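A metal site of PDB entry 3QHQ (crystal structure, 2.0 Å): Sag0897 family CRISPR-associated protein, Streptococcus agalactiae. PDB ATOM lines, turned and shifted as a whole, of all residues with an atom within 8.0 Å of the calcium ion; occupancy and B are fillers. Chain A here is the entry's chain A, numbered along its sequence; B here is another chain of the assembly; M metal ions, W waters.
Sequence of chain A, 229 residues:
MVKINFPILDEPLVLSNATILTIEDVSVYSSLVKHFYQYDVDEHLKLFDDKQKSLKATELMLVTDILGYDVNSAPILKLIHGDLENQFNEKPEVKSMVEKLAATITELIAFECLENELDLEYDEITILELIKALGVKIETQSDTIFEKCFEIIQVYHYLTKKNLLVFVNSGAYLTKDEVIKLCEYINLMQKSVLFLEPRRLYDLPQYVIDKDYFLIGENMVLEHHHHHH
The backbone NH (N) of Asp 123 lies within hydrogen-bond range of the backbone carbonyl oxygen (O) of Leu 134 of chain B, at 2.8 Å.
The backbone NH (N) of Glu 129 sits at hydrogen-bond distance from the side-chain hydroxyl (OG1) of Thr 126, 3.0 Å away.
Four residues have an atom within 4 Å of the calcium ion: Asp 123, Glu 124, Glu 129 and Ala 133 of chain B.
The calcium ion is bound by the backbone carbonyl oxygen (O) of Ala 133 of chain B (2.3 Å), the backbone carbonyl oxygen (O) of Glu 124 (2.3 Å), water W2 (2.4 Å), the side-chain carboxylate (OD1) of Asp 123 (2.4 Å), the side-chain carboxylate (OE2) of Glu 129 (2.5 Å), water W1 (2.5 Å) and the side-chain carboxylate (OE1) of Glu 129 (2.5 Å).
The calcium ion has seven donor atoms within binding distance.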
ATOM      1  N   TYR A 122       8.474   0.575   9.475  1.00  0.00           N
ATOM      2  CA  TYR A 122       8.312   0.403  10.926  1.00  0.00           C
ATOM      3  C   TYR A 122       8.811   1.642  11.655  1.00  0.00           C
ATOM      4  O   TYR A 122       9.382   2.556  11.037  1.00  0.00           O
ATOM      5  CB  TYR A 122       9.058  -0.850  11.413  1.00  0.00           C
ATOM      6  CG  TYR A 122      10.497  -0.915  10.991  1.00  0.00           C
ATOM      7  CD1 TYR A 122      11.488  -0.222  11.687  1.00  0.00           C
ATOM      8  CD2 TYR A 122      10.883  -1.652   9.876  1.00  0.00           C
ATOM      9  CE1 TYR A 122      12.815  -0.266  11.284  1.00  0.00           C
ATOM     10  CE2 TYR A 122      12.204  -1.713   9.461  1.00  0.00           C
ATOM     11  CZ  TYR A 122      13.165  -1.021  10.179  1.00  0.00           C
ATOM     12  OH  TYR A 122      14.471  -1.064   9.770  1.00  0.00           O
ATOM     13  N   ASP A 123       8.584   1.701  12.967  1.00  0.00           N
ATOM     14  CA  ASP A 123       9.126   2.802  13.768  1.00  0.00           C
ATOM     15  C   ASP A 123      10.338   2.359  14.616  1.00  0.00           C
ATOM     16  O   ASP A 123      11.427   2.224  14.075  1.00  0.00           O
ATOM     17  CB  ASP A 123       8.040   3.586  14.556  1.00  0.00           C
ATOM     18  CG  ASP A 123       7.105   2.699  15.377  1.00  0.00           C
ATOM     19  OD1 ASP A 123       7.525   2.174  16.422  1.00  0.00           O
ATOM     20  OD2 ASP A 123       5.916   2.596  15.013  1.00  0.00           O
ATOM     21  N   GLU A 124      10.143   2.117  15.920  1.00  0.00           N
ATOM     22  CA  GLU A 124      11.228   1.676  16.802  1.00  0.00           C
ATOM     23  C   GLU A 124      10.672   0.912  17.993  1.00  0.00           C
ATOM     24  O   GLU A 124       9.506   1.065  18.343  1.00  0.00           O
ATOM     25  CB  GLU A 124      12.059   2.878  17.296  1.00  0.00           C
ATOM     26  CG  GLU A 124      11.259   3.902  18.146  1.00  0.00           C
ATOM     27  CD  GLU A 124      10.405   4.822  17.294  1.00  0.00           C
ATOM     28  OE1 GLU A 124      10.915   5.349  16.282  1.00  0.00           O
ATOM     29  OE2 GLU A 124       9.210   5.025  17.637  1.00  0.00           O
ATOM     30  N   ILE A 125      11.531   0.120  18.631  1.00  0.00           N
ATOM     31  CA  ILE A 125      11.165  -0.558  19.871  1.00  0.00           C
ATOM     32  C   ILE A 125      11.731   0.256  21.048  1.00  0.00           C
ATOM     33  O   ILE A 125      12.943   0.375  21.200  1.00  0.00           O
ATOM     34  CB  ILE A 125      11.690  -2.018  19.930  1.00  0.00           C
ATOM     35  CG1 ILE A 125      11.144  -2.827  18.738  1.00  0.00           C
ATOM     36  CG2 ILE A 125      11.317  -2.677  21.273  1.00  0.00           C
ATOM     37  CD1 ILE A 125      11.827  -4.206  18.533  1.00  0.00           C
ATOM     38  N   THR A 126      10.844   0.818  21.859  1.00  0.00           N
ATOM     39  CA  THR A 126      11.280   1.665  22.976  1.00  0.00           C
ATOM     40  C   THR A 126      11.416   0.845  24.250  1.00  0.00           C
ATOM     41  O   THR A 126      10.863  -0.248  24.367  1.00  0.00           O
ATOM     42  CB  THR A 126      10.312   2.818  23.225  1.00  0.00           C
ATOM     43  OG1 THR A 126       9.079   2.291  23.735  1.00  0.00           O
ATOM     44  CG2 THR A 126      10.044   3.606  21.930  1.00  0.00           C
ATOM     45  N   GLU A 129       7.964   0.302  25.706  1.00  0.00           N
ATOM     46  CA  GLU A 129       7.260  -0.780  25.014  1.00  0.00           C
ATOM     47  C   GLU A 129       7.716  -2.153  25.482  1.00  0.00           C
ATOM     48  O   GLU A 129       6.904  -3.077  25.598  1.00  0.00           O
ATOM     49  CB  GLU A 129       7.415  -0.636  23.486  1.00  0.00           C
ATOM     50  CG  GLU A 129       6.533   0.469  22.892  1.00  0.00           C
ATOM     51  CD  GLU A 129       6.796   0.706  21.420  1.00  0.00           C
ATOM     52  OE1 GLU A 129       7.925   0.438  20.930  1.00  0.00           O
ATOM     53  OE2 GLU A 129       5.868   1.180  20.722  1.00  0.00           O
ATOM     54  N   LEU B 130       7.491  -8.205  19.984  1.00  0.00           N
ATOM     55  CA  LEU B 130       8.579  -7.373  19.469  1.00  0.00           C
ATOM     56  C   LEU B 130       8.231  -6.781  18.104  1.00  0.00           C
ATOM     57  O   LEU B 130       8.468  -5.602  17.852  1.00  0.00           O
ATOM     58  CB  LEU B 130       9.890  -8.159  19.418  1.00  0.00           C
ATOM     59  CG  LEU B 130      10.488  -8.517  20.793  1.00  0.00           C
ATOM     60  CD1 LEU B 130      11.526  -9.628  20.672  1.00  0.00           C
ATOM     61  CD2 LEU B 130      11.075  -7.292  21.474  1.00  0.00           C
ATOM     62  N   ILE B 131       7.635  -7.614  17.242  1.00  0.00           N
ATOM     63  CA  ILE B 131       7.174  -7.177  15.921  1.00  0.00           C
ATOM     64  C   ILE B 131       6.105  -6.083  16.033  1.00  0.00           C
ATOM     65  O   ILE B 131       6.188  -5.062  15.343  1.00  0.00           O
ATOM     66  CB  ILE B 131       6.655  -8.376  15.094  1.00  0.00           C
ATOM     67  CG1 ILE B 131       7.809  -9.340  14.781  1.00  0.00           C
ATOM     68  CG2 ILE B 131       5.979  -7.888  13.793  1.00  0.00           C
ATOM     69  CD1 ILE B 131       7.355 -10.726  14.345  1.00  0.00           C
ATOM     70  N   LYS B 132       5.132  -6.300  16.913  1.00  0.00           N
ATOM     71  CA  LYS B 132       4.074  -5.305  17.161  1.00  0.00           C
ATOM     72  C   LYS B 132       4.630  -3.980  17.700  1.00  0.00           C
ATOM     73  O   LYS B 132       4.279  -2.909  17.214  1.00  0.00           O
ATOM     74  CB  LYS B 132       3.024  -5.854  18.145  1.00  0.00           C
ATOM     75  CG  LYS B 132       2.046  -6.841  17.518  1.00  0.00           C
ATOM     76  CD  LYS B 132       1.202  -7.556  18.571  1.00  0.00           C
ATOM     77  CE  LYS B 132       0.213  -8.532  17.920  1.00  0.00           C
ATOM     78  NZ  LYS B 132      -0.525  -9.360  18.918  1.00  0.00           N
ATOM     79  N   ALA B 133       5.514  -4.073  18.688  1.00  0.00           N
ATOM     80  CA  ALA B 133       6.147  -2.900  19.277  1.00  0.00           C
ATOM     81  C   ALA B 133       6.965  -2.141  18.239  1.00  0.00           C
ATOM     82  O   ALA B 133       7.046  -0.928  18.306  1.00  0.00           O
ATOM     83  CB  ALA B 133       7.037  -3.297  20.467  1.00  0.00           C
ATOM     84  N   LEU B 134       7.554  -2.854  17.291  1.00  0.00           N
ATOM     85  CA  LEU B 134       8.315  -2.217  16.211  1.00  0.00           C
ATOM     86  C   LEU B 134       7.413  -1.403  15.268  1.00  0.00           C
ATOM     87  O   LEU B 134       7.903  -0.542  14.541  1.00  0.00           O
ATOM     88  CB  LEU B 134       9.135  -3.252  15.429  1.00  0.00           C
ATOM     89  CG  LEU B 134      10.234  -2.746  14.480  1.00  0.00           C
ATOM     90  CD1 LEU B 134      11.060  -1.606  15.075  1.00  0.00           C
ATOM     91  CD2 LEU B 134      11.141  -3.896  14.077  1.00  0.00           C
ATOM     92  N   GLY B 135       6.113  -1.669  15.295  1.00  0.00           N
ATOM     93  CA  GLY B 135       5.139  -0.904  14.507  1.00  0.00           C
ATOM     94  C   GLY B 135       5.247  -1.199  13.016  1.00  0.00           C
ATOM     95  O   GLY B 135       5.102  -0.296  12.180  1.00  0.00           O
ATOM     96  N   VAL B 136       5.510  -2.462  12.686  1.00  0.00           N
ATOM     97  CA  VAL B 136       5.618  -2.890  11.296  1.00  0.00           C
ATOM     98  C   VAL B 136       4.287  -2.650  10.584  1.00  0.00           C
ATOM     99  O   VAL B 136       3.230  -3.016  11.089  1.00  0.00           O
ATOM    100  CB  VAL B 136       6.036  -4.385  11.164  1.00  0.00           C
ATOM    101  CG1 VAL B 136       6.060  -4.835   9.696  1.00  0.00           C
ATOM    102  CG2 VAL B 136       7.409  -4.611  11.805  1.00  0.00           C
HETATM  103 CA    CA M   1       7.207   1.320  18.665  1.00  0.00          CA
HETATM  104  O   HOH W   1       4.944   1.533  17.628  1.00  0.00           O
HETATM  105  O   HOH W   2       7.567   3.599  19.222  1.00  0.00           O
